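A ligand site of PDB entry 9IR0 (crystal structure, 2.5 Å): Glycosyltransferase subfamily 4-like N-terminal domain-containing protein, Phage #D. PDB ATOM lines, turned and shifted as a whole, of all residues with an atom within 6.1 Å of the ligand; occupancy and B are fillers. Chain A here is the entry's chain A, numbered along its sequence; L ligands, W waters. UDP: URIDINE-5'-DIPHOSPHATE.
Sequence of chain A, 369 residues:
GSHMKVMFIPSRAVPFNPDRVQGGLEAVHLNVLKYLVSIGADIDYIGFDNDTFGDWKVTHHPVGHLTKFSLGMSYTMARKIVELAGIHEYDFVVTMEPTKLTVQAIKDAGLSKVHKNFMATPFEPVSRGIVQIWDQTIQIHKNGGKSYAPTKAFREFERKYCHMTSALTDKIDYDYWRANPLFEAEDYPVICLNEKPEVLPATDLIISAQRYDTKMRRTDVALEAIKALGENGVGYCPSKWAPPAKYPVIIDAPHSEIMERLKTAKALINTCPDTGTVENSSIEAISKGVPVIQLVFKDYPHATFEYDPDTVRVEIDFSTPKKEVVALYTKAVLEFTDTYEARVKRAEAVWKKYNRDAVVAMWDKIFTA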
ATOM      1  N   GLY A  23     -34.868   0.500  -6.884  1.00  0.00           N
ATOM      2  CA  GLY A  23     -34.228  -0.546  -6.101  1.00  0.00           C
ATOM      3  C   GLY A  23     -34.556  -0.413  -4.622  1.00  0.00           C
ATOM      4  O   GLY A  23     -35.620   0.076  -4.248  1.00  0.00           O
ATOM      5  N   SER A 208     -20.675   1.241 -18.385  1.00  0.00           N
ATOM      6  CA  SER A 208     -20.897   1.526 -16.980  1.00  0.00           C
ATOM      7  C   SER A 208     -22.322   2.031 -16.778  1.00  0.00           C
ATOM      8  O   SER A 208     -22.679   3.086 -17.295  1.00  0.00           O
ATOM      9  CB  SER A 208     -19.897   2.552 -16.465  1.00  0.00           C
ATOM     10  OG  SER A 208     -20.182   2.909 -15.116  1.00  0.00           O
ATOM     11  N   ALA A 209     -23.124   1.256 -16.040  1.00  0.00           N
ATOM     12  CA  ALA A 209     -24.480   1.652 -15.677  1.00  0.00           C
ATOM     13  C   ALA A 209     -24.538   1.922 -14.178  1.00  0.00           C
ATOM     14  O   ALA A 209     -25.113   1.142 -13.421  1.00  0.00           O
ATOM     15  CB  ALA A 209     -25.470   0.563 -16.072  1.00  0.00           C
ATOM     16  N   GLN A 210     -23.929   3.034 -13.763  1.00  0.00           N
ATOM     17  CA  GLN A 210     -23.765   3.374 -12.360  1.00  0.00           C
ATOM     18  C   GLN A 210     -24.080   4.841 -12.098  1.00  0.00           C
ATOM     19  O   GLN A 210     -23.767   5.701 -12.912  1.00  0.00           O
ATOM     20  CB  GLN A 210     -22.319   3.097 -11.909  1.00  0.00           C
ATOM     21  CG  GLN A 210     -21.892   1.633 -12.053  1.00  0.00           C
ATOM     22  CD  GLN A 210     -20.487   1.420 -11.557  1.00  0.00           C
ATOM     23  OE1 GLN A 210     -20.261   0.798 -10.504  1.00  0.00           O
ATOM     24  NE2 GLN A 210     -19.519   1.933 -12.281  1.00  0.00           N
ATOM     25  N   ARG A 211     -24.703   5.105 -10.943  1.00  0.00           N
ATOM     26  CA  ARG A 211     -24.821   6.460 -10.426  1.00  0.00           C
ATOM     27  C   ARG A 211     -23.428   7.059 -10.280  1.00  0.00           C
ATOM     28  O   ARG A 211     -22.491   6.345  -9.948  1.00  0.00           O
ATOM     29  CB  ARG A 211     -25.500   6.462  -9.046  1.00  0.00           C
ATOM     30  CG  ARG A 211     -26.945   5.987  -9.025  1.00  0.00           C
ATOM     31  CD  ARG A 211     -27.474   5.900  -7.601  1.00  0.00           C
ATOM     32  NE  ARG A 211     -26.721   4.934  -6.807  1.00  0.00           N
ATOM     33  CZ  ARG A 211     -25.899   5.251  -5.804  1.00  0.00           C
ATOM     34  NH1 ARG A 211     -25.753   6.496  -5.392  1.00  0.00           N
ATOM     35  NH2 ARG A 211     -25.211   4.283  -5.203  1.00  0.00           N
ATOM     36  N   ARG A 217     -19.593   4.204  -5.065  1.00  0.00           N
ATOM     37  CA  ARG A 217     -19.390   3.411  -6.274  1.00  0.00           C
ATOM     38  C   ARG A 217     -18.135   3.759  -7.070  1.00  0.00           C
ATOM     39  O   ARG A 217     -17.877   3.140  -8.101  1.00  0.00           O
ATOM     40  CB  ARG A 217     -20.611   3.552  -7.204  1.00  0.00           C
ATOM     41  CG  ARG A 217     -21.904   3.022  -6.611  1.00  0.00           C
ATOM     42  CD  ARG A 217     -22.920   2.702  -7.706  1.00  0.00           C
ATOM     43  NE  ARG A 217     -22.520   1.531  -8.478  1.00  0.00           N
ATOM     44  CZ  ARG A 217     -22.556   0.282  -8.028  1.00  0.00           C
ATOM     45  NH1 ARG A 217     -23.213  -0.039  -6.918  1.00  0.00           N
ATOM     46  NH2 ARG A 217     -21.936  -0.674  -8.719  1.00  0.00           N
ATOM     47  N   TYR A 236     -23.647   5.314 -18.579  1.00  0.00           N
ATOM     48  CA  TYR A 236     -25.018   5.729 -18.311  1.00  0.00           C
ATOM     49  C   TYR A 236     -25.103   6.195 -16.857  1.00  0.00           C
ATOM     50  O   TYR A 236     -24.641   5.504 -15.959  1.00  0.00           O
ATOM     51  CB  TYR A 236     -26.008   4.580 -18.566  1.00  0.00           C
ATOM     52  CG  TYR A 236     -26.117   4.166 -20.009  1.00  0.00           C
ATOM     53  CD1 TYR A 236     -26.863   4.919 -20.918  1.00  0.00           C
ATOM     54  CD2 TYR A 236     -25.444   3.052 -20.491  1.00  0.00           C
ATOM     55  CE1 TYR A 236     -26.950   4.549 -22.259  1.00  0.00           C
ATOM     56  CE2 TYR A 236     -25.518   2.673 -21.827  1.00  0.00           C
ATOM     57  CZ  TYR A 236     -26.282   3.432 -22.711  1.00  0.00           C
ATOM     58  OH  TYR A 236     -26.372   3.057 -24.036  1.00  0.00           O
ATOM     59  N   CYS A 237     -25.697   7.379 -16.668  1.00  0.00           N
ATOM     60  CA  CYS A 237     -25.927   7.945 -15.340  1.00  0.00           C
ATOM     61  C   CYS A 237     -27.339   8.541 -15.269  1.00  0.00           C
ATOM     62  O   CYS A 237     -27.812   9.109 -16.249  1.00  0.00           O
ATOM     63  CB  CYS A 237     -24.885   9.007 -15.005  1.00  0.00           C
ATOM     64  SG  CYS A 237     -23.212   8.360 -14.768  1.00  0.00           S
ATOM     65  N   PRO A 238     -28.042   8.415 -14.126  1.00  0.00           N
ATOM     66  CA  PRO A 238     -29.259   9.191 -13.910  1.00  0.00           C
ATOM     67  C   PRO A 238     -28.948  10.655 -13.631  1.00  0.00           C
ATOM     68  O   PRO A 238     -27.864  10.978 -13.151  1.00  0.00           O
ATOM     69  CB  PRO A 238     -29.918   8.488 -12.720  1.00  0.00           C
ATOM     70  CG  PRO A 238     -28.782   7.852 -11.982  1.00  0.00           C
ATOM     71  CD  PRO A 238     -27.716   7.529 -12.993  1.00  0.00           C
ATOM     72  N   ILE A 250     -24.516   9.340 -21.011  1.00  0.00           N
ATOM     73  CA  ILE A 250     -25.905   9.458 -21.423  1.00  0.00           C
ATOM     74  C   ILE A 250     -26.771   9.580 -20.180  1.00  0.00           C
ATOM     75  O   ILE A 250     -26.775   8.693 -19.329  1.00  0.00           O
ATOM     76  CB  ILE A 250     -26.308   8.271 -22.327  1.00  0.00           C
ATOM     77  CG1 ILE A 250     -25.707   8.439 -23.746  1.00  0.00           C
ATOM     78  CG2 ILE A 250     -27.823   8.099 -22.391  1.00  0.00           C
ATOM     79  CD1 ILE A 250     -25.561   7.170 -24.545  1.00  0.00           C
ATOM     80  N   ILE A 251     -27.515  10.696 -20.091  1.00  0.00           N
ATOM     81  CA  ILE A 251     -28.305  11.026 -18.910  1.00  0.00           C
ATOM     82  C   ILE A 251     -29.729  10.494 -19.034  1.00  0.00           C
ATOM     83  O   ILE A 251     -30.370  10.688 -20.063  1.00  0.00           O
ATOM     84  CB  ILE A 251     -28.317  12.557 -18.664  1.00  0.00           C
ATOM     85  CG1 ILE A 251     -26.906  13.175 -18.740  1.00  0.00           C
ATOM     86  CG2 ILE A 251     -29.000  12.887 -17.336  1.00  0.00           C
ATOM     87  CD1 ILE A 251     -25.791  12.314 -18.170  1.00  0.00           C
ATOM     88  N   ASP A 252     -30.219   9.835 -17.971  1.00  0.00           N
ATOM     89  CA  ASP A 252     -31.591   9.368 -17.904  1.00  0.00           C
ATOM     90  C   ASP A 252     -32.056   8.681 -19.183  1.00  0.00           C
ATOM     91  O   ASP A 252     -33.086   9.036 -19.742  1.00  0.00           O
ATOM     92  CB  ASP A 252     -32.535  10.531 -17.569  1.00  0.00           C
ATOM     93  CG  ASP A 252     -32.489  11.028 -16.133  1.00  0.00           C
ATOM     94  OD1 ASP A 252     -31.941  10.312 -15.283  1.00  0.00           O
ATOM     95  OD2 ASP A 252     -33.015  12.133 -15.878  1.00  0.00           O
ATOM     96  N   ALA A 253     -31.272   7.692 -19.636  1.00  0.00           N
ATOM     97  CA  ALA A 253     -31.692   6.849 -20.739  1.00  0.00           C
ATOM     98  C   ALA A 253     -32.790   5.908 -20.237  1.00  0.00           C
ATOM     99  O   ALA A 253     -32.708   5.423 -19.113  1.00  0.00           O
ATOM    100  CB  ALA A 253     -30.526   6.055 -21.295  1.00  0.00           C
ATOM    101  N   HIS A 255     -34.439   2.691 -19.201  1.00  0.00           N
ATOM    102  CA  HIS A 255     -33.777   1.485 -18.736  1.00  0.00           C
ATOM    103  C   HIS A 255     -33.754   0.393 -19.808  1.00  0.00           C
ATOM    104  O   HIS A 255     -32.735  -0.272 -19.984  1.00  0.00           O
ATOM    105  CB  HIS A 255     -34.454   0.937 -17.462  1.00  0.00           C
ATOM    106  CG  HIS A 255     -33.744  -0.241 -16.872  1.00  0.00           C
ATOM    107  ND1 HIS A 255     -32.537  -0.088 -16.222  1.00  0.00           N
ATOM    108  CD2 HIS A 255     -34.082  -1.539 -16.857  1.00  0.00           C
ATOM    109  CE1 HIS A 255     -32.178  -1.297 -15.829  1.00  0.00           C
ATOM    110  NE2 HIS A 255     -33.085  -2.209 -16.197  1.00  0.00           N
ATOM    111  N   ILE A 258     -30.879   0.716 -22.205  1.00  0.00           N
ATOM    112  CA  ILE A 258     -29.613   0.329 -21.606  1.00  0.00           C
ATOM    113  C   ILE A 258     -29.469  -1.187 -21.674  1.00  0.00           C
ATOM    114  O   ILE A 258     -28.436  -1.703 -22.084  1.00  0.00           O
ATOM    115  CB  ILE A 258     -29.470   0.838 -20.145  1.00  0.00           C
ATOM    116  CG1 ILE A 258     -29.720   2.358 -20.033  1.00  0.00           C
ATOM    117  CG2 ILE A 258     -28.101   0.453 -19.560  1.00  0.00           C
ATOM    118  CD1 ILE A 258     -29.596   2.916 -18.631  1.00  0.00           C
ATOM    119  N   MET A 259     -30.535  -1.886 -21.272  1.00  0.00           N
ATOM    120  CA  MET A 259     -30.561  -3.341 -21.248  1.00  0.00           C
ATOM    121  C   MET A 259     -30.385  -3.911 -22.648  1.00  0.00           C
ATOM    122  O   MET A 259     -29.660  -4.886 -22.841  1.00  0.00           O
ATOM    123  CB  MET A 259     -31.890  -3.836 -20.647  1.00  0.00           C
ATOM    124  CG  MET A 259     -32.113  -3.454 -19.184  1.00  0.00           C
ATOM    125  SD  MET A 259     -31.055  -4.346 -18.026  1.00  0.00           S
ATOM    126  CE  MET A 259     -29.810  -3.088 -17.696  1.00  0.00           C
ATOM    127  N   CYS A 272     -17.859  -0.509  -7.559  1.00  0.00           N
ATOM    128  CA  CYS A 272     -18.194  -0.502  -6.138  1.00  0.00           C
ATOM    129  C   CYS A 272     -17.429  -1.625  -5.436  1.00  0.00           C
ATOM    130  O   CYS A 272     -17.799  -2.784  -5.578  1.00  0.00           O
ATOM    131  CB  CYS A 272     -19.691  -0.641  -5.928  1.00  0.00           C
ATOM    132  SG  CYS A 272     -20.182  -0.860  -4.187  1.00  0.00           S
ATOM    133  N   VAL A 278     -26.066  -6.148  -3.275  1.00  0.00           N
ATOM    134  CA  VAL A 278     -27.070  -6.585  -4.215  1.00  0.00           C
ATOM    135  C   VAL A 278     -26.539  -6.469  -5.645  1.00  0.00           C
ATOM    136  O   VAL A 278     -26.516  -7.457  -6.369  1.00  0.00           O
ATOM    137  CB  VAL A 278     -28.375  -5.780  -4.026  1.00  0.00           C
ATOM    138  CG1 VAL A 278     -29.212  -5.771  -5.302  1.00  0.00           C
ATOM    139  CG2 VAL A 278     -29.181  -6.306  -2.850  1.00  0.00           C
ATOM    140  N   GLU A 279     -26.141  -5.253  -6.036  1.00  0.00           N
ATOM    141  CA  GLU A 279     -25.522  -4.983  -7.323  1.00  0.00           C
ATOM    142  C   GLU A 279     -26.395  -5.459  -8.484  1.00  0.00           C
ATOM    143  O   GLU A 279     -26.091  -6.470  -9.125  1.00  0.00           O
ATOM    144  CB  GLU A 279     -24.134  -5.616  -7.380  1.00  0.00           C
ATOM    145  CG  GLU A 279     -23.243  -5.160  -6.255  1.00  0.00           C
ATOM    146  CD  GLU A 279     -22.973  -3.663  -6.232  1.00  0.00           C
ATOM    147  OE1 GLU A 279     -23.769  -2.923  -5.617  1.00  0.00           O
ATOM    148  OE2 GLU A 279     -21.965  -3.238  -6.840  1.00  0.00           O
ATOM    149  N   ASN A 280     -27.463  -4.711  -8.747  1.00  0.00           N
ATOM    150  CA  ASN A 280     -28.432  -5.047  -9.774  1.00  0.00           C
ATOM    151  C   ASN A 280     -27.855  -5.021 -11.183  1.00  0.00           C
ATOM    152  O   ASN A 280     -28.201  -5.863 -12.010  1.00  0.00           O
ATOM    153  CB  ASN A 280     -29.650  -4.128  -9.689  1.00  0.00           C
ATOM    154  CG  ASN A 280     -30.449  -4.357  -8.438  1.00  0.00           C
ATOM    155  OD1 ASN A 280     -30.417  -3.540  -7.517  1.00  0.00           O
ATOM    156  ND2 ASN A 280     -31.139  -5.476  -8.341  1.00  0.00           N
ATOM    157  N   SER A 281     -26.968  -4.048 -11.465  1.00  0.00           N
ATOM    158  CA  SER A 281     -26.407  -3.922 -12.806  1.00  0.00           C
ATOM    159  C   SER A 281     -25.512  -5.106 -13.151  1.00  0.00           C
ATOM    160  O   SER A 281     -25.410  -5.463 -14.320  1.00  0.00           O
ATOM    161  CB  SER A 281     -25.661  -2.597 -12.975  1.00  0.00           C
ATOM    162  OG  SER A 281     -24.344  -2.623 -12.449  1.00  0.00           O
ATOM    163  N   SER A 282     -24.910  -5.733 -12.131  1.00  0.00           N
ATOM    164  CA  SER A 282     -24.115  -6.939 -12.330  1.00  0.00           C
ATOM    165  C   SER A 282     -24.956  -8.120 -12.821  1.00  0.00           C
ATOM    166  O   SER A 282     -24.581  -8.789 -13.779  1.00  0.00           O
ATOM    167  CB  SER A 282     -23.383  -7.333 -11.048  1.00  0.00           C
ATOM    168  OG  SER A 282     -22.327  -6.432 -10.781  1.00  0.00           O
ATOM    169  N   GLU A 284     -27.943  -7.843 -14.080  1.00  0.00           N
ATOM    170  CA  GLU A 284     -28.489  -7.393 -15.350  1.00  0.00           C
ATOM    171  C   GLU A 284     -27.583  -7.803 -16.502  1.00  0.00           C
ATOM    172  O   GLU A 284     -28.060  -8.276 -17.534  1.00  0.00           O
ATOM    173  CB  GLU A 284     -28.703  -5.868 -15.345  1.00  0.00           C
ATOM    174  CG  GLU A 284     -29.963  -5.427 -14.604  1.00  0.00           C
ATOM    175  CD  GLU A 284     -30.108  -3.936 -14.338  1.00  0.00           C
ATOM    176  OE1 GLU A 284     -29.152  -3.182 -14.616  1.00  0.00           O
ATOM    177  OE2 GLU A 284     -31.188  -3.534 -13.856  1.00  0.00           O
HETATM  178  N1  UDP L   1     -29.416   2.477 -13.909  1.00  0.00           N
HETATM  179  C2  UDP L   1     -30.338   3.144 -14.691  1.00  0.00           C
HETATM  180  N3  UDP L   1     -29.856   4.225 -15.373  1.00  0.00           N
HETATM  181  C4  UDP L   1     -28.568   4.706 -15.352  1.00  0.00           C
HETATM  182  C5  UDP L   1     -27.661   3.969 -14.519  1.00  0.00           C
HETATM  183  C6  UDP L   1     -28.106   2.906 -13.843  1.00  0.00           C
HETATM  184  O2  UDP L   1     -31.508   2.795 -14.779  1.00  0.00           O
HETATM  185  O4  UDP L   1     -28.273   5.704 -16.027  1.00  0.00           O
HETATM  186  C1' UDP L   1     -29.883   1.303 -13.142  1.00  0.00           C
HETATM  187  C2' UDP L   1     -29.024   0.052 -13.343  1.00  0.00           C
HETATM  188  O2' UDP L   1     -29.416  -0.616 -14.529  1.00  0.00           O
HETATM  189  C3' UDP L   1     -29.342  -0.704 -12.048  1.00  0.00           C
HETATM  190  C4' UDP L   1     -29.342   0.437 -11.028  1.00  0.00           C
HETATM  191  O4' UDP L   1     -29.837   1.590 -11.765  1.00  0.00           O
HETATM  192  O3' UDP L   1     -30.609  -1.353 -12.076  1.00  0.00           O
HETATM  193  C5' UDP L   1     -28.014   0.783 -10.409  1.00  0.00           C
HETATM  194  O5' UDP L   1     -27.310  -0.424 -10.026  1.00  0.00           O
HETATM  195  PA  UDP L   1     -27.469  -0.953  -8.528  1.00  0.00           P
HETATM  196  O1A UDP L   1     -28.889  -0.752  -8.089  1.00  0.00           O
HETATM  197  O2A UDP L   1     -26.880  -2.320  -8.408  1.00  0.00           O
HETATM  198  O3A UDP L   1     -26.523   0.059  -7.738  1.00  0.00           O
HETATM  199  PB  UDP L   1     -26.846   1.126  -6.570  1.00  0.00           P
HETATM  200  O1B UDP L   1     -27.328   2.354  -7.294  1.00  0.00           O
HETATM  201  O2B UDP L   1     -27.903   0.490  -5.689  1.00  0.00           O
HETATM  202  O3B UDP L   1     -25.528   1.335  -5.837  1.00  0.00           O
HETATM  203  O   HOH W   1     -25.704   2.488  -9.558  1.00  0.00           O
HETATM  204  O   HOH W   2     -24.852  -2.795 -10.002  1.00  0.00           O
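The backbone NH (N) of Asn 280 is in hydrogen-bond range of an oxygen (O2A) of the ligand (2.5 Å).
The side-chain amide oxygen (OD1) of Asn 280 sits close to an oxygen (O1A) of the ligand (3.2 Å).
The side-chain carboxylate (OE1) of Glu 284 is in hydrogen-bond range of an oxygen (O2') of the ligand (2.6 Å).
An oxygen (O1B) of the ligand is in salt-bridge range of the guanidinium group (NE) of Arg 211 (2.7 Å).
The guanidinium group (NH1) of Arg 217 is in salt-bridge range of an oxygen (O3B) of the ligand.
The backbone NH (N) of Cys 237 sits close to an oxygen (O4) of the ligand.
An oxygen (O2) of the ligand is in hydrogen-bond range of a ring nitrogen (ND1) of His 255 (3.4 Å).
The side-chain carboxylate (OE2) of Glu 279 is in salt-bridge range of the guanidinium group (NH2) of Arg 217, 3.2 Å away.
The side-chain amide oxygen (OE1) of Gln 210 sits at hydrogen-bond distance from the guanidinium group (NH2) of Arg 217 (2.9 Å).
O of Gln 210 is in hydrogen-bond range of SG of Cys 237, at 3.3 Å.
O of Ile 250 is in hydrogen-bond range of N of Cys 237, at 3.2 Å.
The backbone carbonyl oxygen of Cys 237 is in hydrogen-bond range of the backbone NH of Asp 252 (3.0 Å).
NE2 of His 255 sits close to SD of Met 259 (3.5 Å).
The backbone NH (N) of Tyr 236 is in hydrogen-bond range of the backbone carbonyl oxygen (O) of Ser 208.
The side-chain amide nitrogen (NE2) of Gln 210 lies within hydrogen-bond range of the side-chain hydroxyl (OG) of Ser 208.
Water W2 lies within hydrogen-bond range of the side-chain hydroxyl of Ser 281, an oxygen (O2A) of the ligand and the backbone NH of Asn 280.
Water W1 lies within hydrogen-bond range of O1B of the ligand (2.8 Å), N of Arg 211 (3.1 Å) and NE of Arg 217 (3.5 Å).
N of Pro 238 sits close to O4 of the ligand (3.3 Å).
Merely in contact with the ligand: Ala 209, Gln 210, Tyr 236, Ile 258, Glu 279 and Ser 281.
Hydrophobic or aromatic side chains that line the ligand: Tyr 236, Pro 238, His 255 and Ile 258.
Within 4 Å of the ligand: Ala 209, Gln 210, Arg 211, Arg 217, Tyr 236, Cys 237, Pro 238, His 255, Ile 258, Glu 279, Asn 280, Ser 281 and Glu 284.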
